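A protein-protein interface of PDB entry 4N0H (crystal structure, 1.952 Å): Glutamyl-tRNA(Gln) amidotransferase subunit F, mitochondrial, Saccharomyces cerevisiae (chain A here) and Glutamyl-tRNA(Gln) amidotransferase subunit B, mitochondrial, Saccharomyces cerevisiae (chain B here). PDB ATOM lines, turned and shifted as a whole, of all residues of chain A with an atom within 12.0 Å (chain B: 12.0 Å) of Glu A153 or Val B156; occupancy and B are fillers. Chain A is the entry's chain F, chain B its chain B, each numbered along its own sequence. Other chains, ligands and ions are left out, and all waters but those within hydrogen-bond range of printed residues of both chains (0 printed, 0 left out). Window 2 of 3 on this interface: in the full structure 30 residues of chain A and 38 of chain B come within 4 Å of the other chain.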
ATOM      1  N   GLU A 143       0.224 -21.137   9.428  1.00  0.00           N
ATOM      2  CA  GLU A 143      -0.499 -20.401   8.399  1.00  0.00           C
ATOM      3  C   GLU A 143       0.367 -20.170   7.169  1.00  0.00           C
ATOM      4  O   GLU A 143       1.590 -20.060   7.265  1.00  0.00           O
ATOM      5  CB  GLU A 143      -0.998 -19.058   8.937  1.00  0.00           C
ATOM      6  CG  GLU A 143      -1.855 -19.167  10.193  1.00  0.00           C
ATOM      7  CD  GLU A 143      -2.576 -17.876  10.518  1.00  0.00           C
ATOM      8  OE1 GLU A 143      -2.981 -17.169   9.569  1.00  0.00           O
ATOM      9  OE2 GLU A 143      -2.733 -17.564  11.720  1.00  0.00           O
ATOM     10  N   LYS A 145      -0.185 -18.869   2.592  1.00  0.00           N
ATOM     11  CA  LYS A 145      -1.058 -18.664   1.446  1.00  0.00           C
ATOM     12  C   LYS A 145      -0.445 -19.316   0.219  1.00  0.00           C
ATOM     13  O   LYS A 145       0.551 -18.829  -0.323  1.00  0.00           O
ATOM     14  CB  LYS A 145      -1.331 -17.183   1.188  1.00  0.00           C
ATOM     15  CG  LYS A 145      -2.343 -16.971   0.069  1.00  0.00           C
ATOM     16  CD  LYS A 145      -2.876 -15.554   0.034  1.00  0.00           C
ATOM     17  CE  LYS A 145      -3.977 -15.419  -1.006  1.00  0.00           C
ATOM     18  NZ  LYS A 145      -4.677 -14.111  -0.902  1.00  0.00           N
ATOM     19  N   PHE A 149       4.899 -17.958   2.728  1.00  0.00           N
ATOM     20  CA  PHE A 149       4.722 -17.674   4.145  1.00  0.00           C
ATOM     21  C   PHE A 149       3.989 -16.341   4.250  1.00  0.00           C
ATOM     22  O   PHE A 149       4.072 -15.510   3.341  1.00  0.00           O
ATOM     23  CB  PHE A 149       6.074 -17.587   4.861  1.00  0.00           C
ATOM     24  CG  PHE A 149       6.839 -18.881   4.882  1.00  0.00           C
ATOM     25  CD1 PHE A 149       6.458 -19.916   5.725  1.00  0.00           C
ATOM     26  CD2 PHE A 149       7.941 -19.065   4.061  1.00  0.00           C
ATOM     27  CE1 PHE A 149       7.162 -21.107   5.750  1.00  0.00           C
ATOM     28  CE2 PHE A 149       8.647 -20.250   4.074  1.00  0.00           C
ATOM     29  CZ  PHE A 149       8.255 -21.279   4.922  1.00  0.00           C
ATOM     30  N   VAL A 150       3.267 -16.129   5.345  1.00  0.00           N
ATOM     31  CA  VAL A 150       2.515 -14.888   5.507  1.00  0.00           C
ATOM     32  C   VAL A 150       2.830 -14.156   6.806  1.00  0.00           C
ATOM     33  O   VAL A 150       2.999 -14.769   7.861  1.00  0.00           O
ATOM     34  CB  VAL A 150       0.985 -15.113   5.396  1.00  0.00           C
ATOM     35  CG1 VAL A 150       0.611 -15.561   3.988  1.00  0.00           C
ATOM     36  CG2 VAL A 150       0.511 -16.126   6.431  1.00  0.00           C
ATOM     37  N   VAL A 151       2.916 -12.834   6.711  1.00  0.00           N
ATOM     38  CA  VAL A 151       3.073 -11.980   7.880  1.00  0.00           C
ATOM     39  C   VAL A 151       1.981 -10.912   7.853  1.00  0.00           C
ATOM     40  O   VAL A 151       1.726 -10.306   6.814  1.00  0.00           O
ATOM     41  CB  VAL A 151       4.462 -11.310   7.918  1.00  0.00           C
ATOM     42  CG1 VAL A 151       4.634 -10.509   9.203  1.00  0.00           C
ATOM     43  CG2 VAL A 151       5.569 -12.355   7.796  1.00  0.00           C
ATOM     44  N   LYS A 152       1.332 -10.690   8.991  1.00  0.00           N
ATOM     45  CA  LYS A 152       0.212  -9.751   9.060  1.00  0.00           C
ATOM     46  C   LYS A 152       0.647  -8.352   9.494  1.00  0.00           C
ATOM     47  O   LYS A 152       1.392  -8.194  10.459  1.00  0.00           O
ATOM     48  CB  LYS A 152      -0.861 -10.277  10.011  1.00  0.00           C
ATOM     49  CG  LYS A 152      -1.289 -11.706   9.735  1.00  0.00           C
ATOM     50  CD  LYS A 152      -1.965 -12.310  10.955  1.00  0.00           C
ATOM     51  CE  LYS A 152      -2.172 -13.810  10.797  1.00  0.00           C
ATOM     52  NZ  LYS A 152      -2.799 -14.415  12.008  1.00  0.00           N
ATOM     53  N   GLU A 153       0.170  -7.337   8.781  1.00  0.00           N
ATOM     54  CA  GLU A 153       0.464  -5.953   9.135  1.00  0.00           C
ATOM     55  C   GLU A 153      -0.262  -5.554  10.416  1.00  0.00           C
ATOM     56  O   GLU A 153      -1.423  -5.912  10.618  1.00  0.00           O
ATOM     57  CB  GLU A 153       0.068  -5.011   7.997  1.00  0.00           C
ATOM     58  N   TYR B  95      12.382  -9.543  10.916  1.00  0.00           N
ATOM     59  CA  TYR B  95      11.640  -9.226   9.703  1.00  0.00           C
ATOM     60  C   TYR B  95      11.215 -10.524   9.038  1.00  0.00           C
ATOM     61  O   TYR B  95      11.908 -11.531   9.146  1.00  0.00           O
ATOM     62  CB  TYR B  95      12.482  -8.384   8.741  1.00  0.00           C
ATOM     63  CG  TYR B  95      11.674  -7.361   7.979  1.00  0.00           C
ATOM     64  CD1 TYR B  95      11.073  -6.296   8.639  1.00  0.00           C
ATOM     65  CD2 TYR B  95      11.510  -7.454   6.602  1.00  0.00           C
ATOM     66  CE1 TYR B  95      10.330  -5.357   7.953  1.00  0.00           C
ATOM     67  CE2 TYR B  95      10.768  -6.516   5.904  1.00  0.00           C
ATOM     68  CZ  TYR B  95      10.181  -5.469   6.586  1.00  0.00           C
ATOM     69  OH  TYR B  95       9.440  -4.526   5.904  1.00  0.00           O
ATOM     70  N   GLY B  96      10.080 -10.495   8.348  1.00  0.00           N
ATOM     71  CA  GLY B  96       9.532 -11.687   7.722  1.00  0.00           C
ATOM     72  C   GLY B  96      10.450 -12.369   6.720  1.00  0.00           C
ATOM     73  O   GLY B  96      10.408 -13.589   6.562  1.00  0.00           O
ATOM     74  N   SER B 147       9.749 -10.031  -0.055  1.00  0.00           N
ATOM     75  CA  SER B 147       8.436  -9.746   0.506  1.00  0.00           C
ATOM     76  C   SER B 147       7.527  -9.127  -0.545  1.00  0.00           C
ATOM     77  O   SER B 147       7.934  -8.224  -1.276  1.00  0.00           O
ATOM     78  CB  SER B 147       8.554  -8.801   1.702  1.00  0.00           C
ATOM     79  OG  SER B 147       9.194  -9.432   2.796  1.00  0.00           O
ATOM     80  N   HIS B 148       6.297  -9.623  -0.622  1.00  0.00           N
ATOM     81  CA  HIS B 148       5.300  -9.075  -1.531  1.00  0.00           C
ATOM     82  C   HIS B 148       4.116  -8.587  -0.713  1.00  0.00           C
ATOM     83  O   HIS B 148       3.432  -9.375  -0.061  1.00  0.00           O
ATOM     84  CB  HIS B 148       4.840 -10.133  -2.537  1.00  0.00           C
ATOM     85  CG  HIS B 148       5.966 -10.857  -3.209  1.00  0.00           C
ATOM     86  ND1 HIS B 148       6.382 -10.562  -4.490  1.00  0.00           N
ATOM     87  CD2 HIS B 148       6.763 -11.863  -2.776  1.00  0.00           C
ATOM     88  CE1 HIS B 148       7.388 -11.355  -4.817  1.00  0.00           C
ATOM     89  NE2 HIS B 148       7.639 -12.152  -3.793  1.00  0.00           N
ATOM     90  N   TYR B 149       3.882  -7.281  -0.740  1.00  0.00           N
ATOM     91  CA  TYR B 149       2.809  -6.687   0.046  1.00  0.00           C
ATOM     92  C   TYR B 149       1.510  -6.665  -0.746  1.00  0.00           C
ATOM     93  O   TYR B 149       1.441  -6.077  -1.823  1.00  0.00           O
ATOM     94  CB  TYR B 149       3.203  -5.281   0.499  1.00  0.00           C
ATOM     95  CG  TYR B 149       4.564  -5.239   1.160  1.00  0.00           C
ATOM     96  CD1 TYR B 149       4.730  -5.654   2.475  1.00  0.00           C
ATOM     97  CD2 TYR B 149       5.684  -4.799   0.466  1.00  0.00           C
ATOM     98  CE1 TYR B 149       5.971  -5.628   3.083  1.00  0.00           C
ATOM     99  CE2 TYR B 149       6.931  -4.766   1.067  1.00  0.00           C
ATOM    100  CZ  TYR B 149       7.067  -5.183   2.377  1.00  0.00           C
ATOM    101  OH  TYR B 149       8.303  -5.155   2.985  1.00  0.00           O
ATOM    102  N   THR B 150       0.488  -7.327  -0.210  1.00  0.00           N
ATOM    103  CA  THR B 150      -0.813  -7.399  -0.862  1.00  0.00           C
ATOM    104  C   THR B 150      -1.898  -6.800   0.025  1.00  0.00           C
ATOM    105  O   THR B 150      -1.692  -6.603   1.224  1.00  0.00           O
ATOM    106  CB  THR B 150      -1.196  -8.854  -1.205  1.00  0.00           C
ATOM    107  OG1 THR B 150      -1.535  -9.561  -0.006  1.00  0.00           O
ATOM    108  CG2 THR B 150      -0.047  -9.561  -1.904  1.00  0.00           C
ATOM    109  N   VAL B 156      -4.305  -6.106   5.453  1.00  0.00           N
ATOM    110  CA  VAL B 156      -3.044  -6.174   4.722  1.00  0.00           C
ATOM    111  C   VAL B 156      -2.167  -7.327   5.204  1.00  0.00           C
ATOM    112  O   VAL B 156      -1.861  -7.439   6.392  1.00  0.00           O
ATOM    113  CB  VAL B 156      -2.256  -4.843   4.809  1.00  0.00           C
ATOM    114  CG1 VAL B 156      -0.791  -5.059   4.462  1.00  0.00           C
ATOM    115  CG2 VAL B 156      -2.872  -3.801   3.889  1.00  0.00           C
ATOM    116  N   ILE B 157      -1.773  -8.185   4.269  1.00  0.00           N
ATOM    117  CA  ILE B 157      -0.897  -9.311   4.563  1.00  0.00           C
ATOM    118  C   ILE B 157       0.291  -9.291   3.603  1.00  0.00           C
ATOM    119  O   ILE B 157       0.141  -8.954   2.428  1.00  0.00           O
ATOM    120  CB  ILE B 157      -1.667 -10.659   4.484  1.00  0.00           C
ATOM    121  CG1 ILE B 157      -1.689 -11.343   5.852  1.00  0.00           C
ATOM    122  CG2 ILE B 157      -1.073 -11.589   3.432  1.00  0.00           C
ATOM    123  CD1 ILE B 157      -2.455 -12.651   5.868  1.00  0.00           C
ATOM    124  N   THR B 158       1.477  -9.618   4.104  1.00  0.00           N
ATOM    125  CA  THR B 158       2.657  -9.651   3.244  1.00  0.00           C
ATOM    126  C   THR B 158       3.130 -11.079   2.990  1.00  0.00           C
ATOM    127  O   THR B 158       3.230 -11.887   3.915  1.00  0.00           O
ATOM    128  CB  THR B 158       3.801  -8.761   3.778  1.00  0.00           C
ATOM    129  OG1 THR B 158       5.023  -9.509   3.819  1.00  0.00           O
ATOM    130  CG2 THR B 158       3.475  -8.236   5.164  1.00  0.00           C
ATOM    131  N   LEU B 159       3.393 -11.379   1.721  1.00  0.00           N
ATOM    132  CA  LEU B 159       3.791 -12.716   1.289  1.00  0.00           C
ATOM    133  C   LEU B 159       5.311 -12.830   1.240  1.00  0.00           C
ATOM    134  O   LEU B 159       5.985 -11.961   0.690  1.00  0.00           O
ATOM    135  CB  LEU B 159       3.211 -13.019  -0.094  1.00  0.00           C
ATOM    136  CG  LEU B 159       1.697 -12.860  -0.264  1.00  0.00           C
ATOM    137  CD1 LEU B 159       1.305 -13.028  -1.718  1.00  0.00           C
ATOM    138  CD2 LEU B 159       0.944 -13.842   0.606  1.00  0.00           C
ATOM    139  N   VAL B 160       5.845 -13.906   1.808  1.00  0.00           N
ATOM    140  CA  VAL B 160       7.286 -14.072   1.902  1.00  0.00           C
ATOM    141  C   VAL B 160       7.774 -15.292   1.133  1.00  0.00           C
ATOM    142  O   VAL B 160       7.302 -16.408   1.349  1.00  0.00           O
ATOM    143  CB  VAL B 160       7.744 -14.177   3.379  1.00  0.00           C
ATOM    144  CG1 VAL B 160       9.245 -14.429   3.453  1.00  0.00           C
ATOM    145  CG2 VAL B 160       7.364 -12.913   4.140  1.00  0.00           C
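Printed residues of chain A that touch a printed residue of chain B: Phe A149, Val A150, Val A151, Lys A152 and Glu A153.
Hydrophobic or aromatic side chains of chain A within 4 Å of the printed part of chain B: Phe A149 and Val A150.
Hydrophobic or aromatic side chains of chain B within 4 Å of the printed part of chain A: Val B156, Ile B157, Leu B159 and Val B160.
Along chain B the printed residues that touch a printed residue of chain A span positions 156 to 160.
Among the printed residues, no Asp or Glu carboxylate lies within 4 Å of a Lys or Arg side-chain nitrogen of the other chain.
The backbone NH (N) of Glu A153 is in hydrogen-bond range of the backbone carbonyl oxygen (O) of Val B156 (3.1 Å).
The backbone NH of Thr B158 lies within hydrogen-bond range of the backbone carbonyl oxygen of Val A151 (2.8 Å).
The backbone carbonyl oxygen of Phe A149 lies within hydrogen-bond range of the backbone NH of Val B160, at 2.8 Å.
The backbone NH (N) of Leu B159 sits at hydrogen-bond distance from the backbone carbonyl oxygen (O) of His B148 (2.7 Å).
The backbone carbonyl oxygen (O) of Ile B157 is in hydrogen-bond range of the side-chain hydroxyl (OG1) of Thr B150 (3.0 Å).
NZ of Lys A152 is in salt-bridge range of OE2 of Glu A143, 3.2 Å away.
Phe A149 touches Thr B158 (O to O, 3.8 Å).
Leu B159 touches Phe A149 (CA to O, 3.5 Å).
CA of Val A150 touches O of Thr B158 (3.5 Å).
Val A150 touches Leu B159.
Ile B157 touches Val A151 (CA to O, 3.6 Å).
Lys A152 touches Ile B157.
Glu A153 touches just one residue of chain B: Val B156.
No residue of chain A comes within 4 Å of Thr B150.
Of chain A, only Phe A149, Val A150 and Val A151 come within 4 Å of Thr B158.
Printed residues of chain B within 4 Å of Lys A152: Ile B157 (3.9 Å).
Of the printed residues of chain B, Phe A149 touches Thr B158 (3.8 Å), Leu B159 (3.5 Å) and Val B160 (2.8 Å).
Of the printed residues of chain B, Val A150 touches Thr B158 (3.5 Å) and Leu B159 (3.8 Å).
Printed residues of chain A within 4 Å of Val B160: Phe A149.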
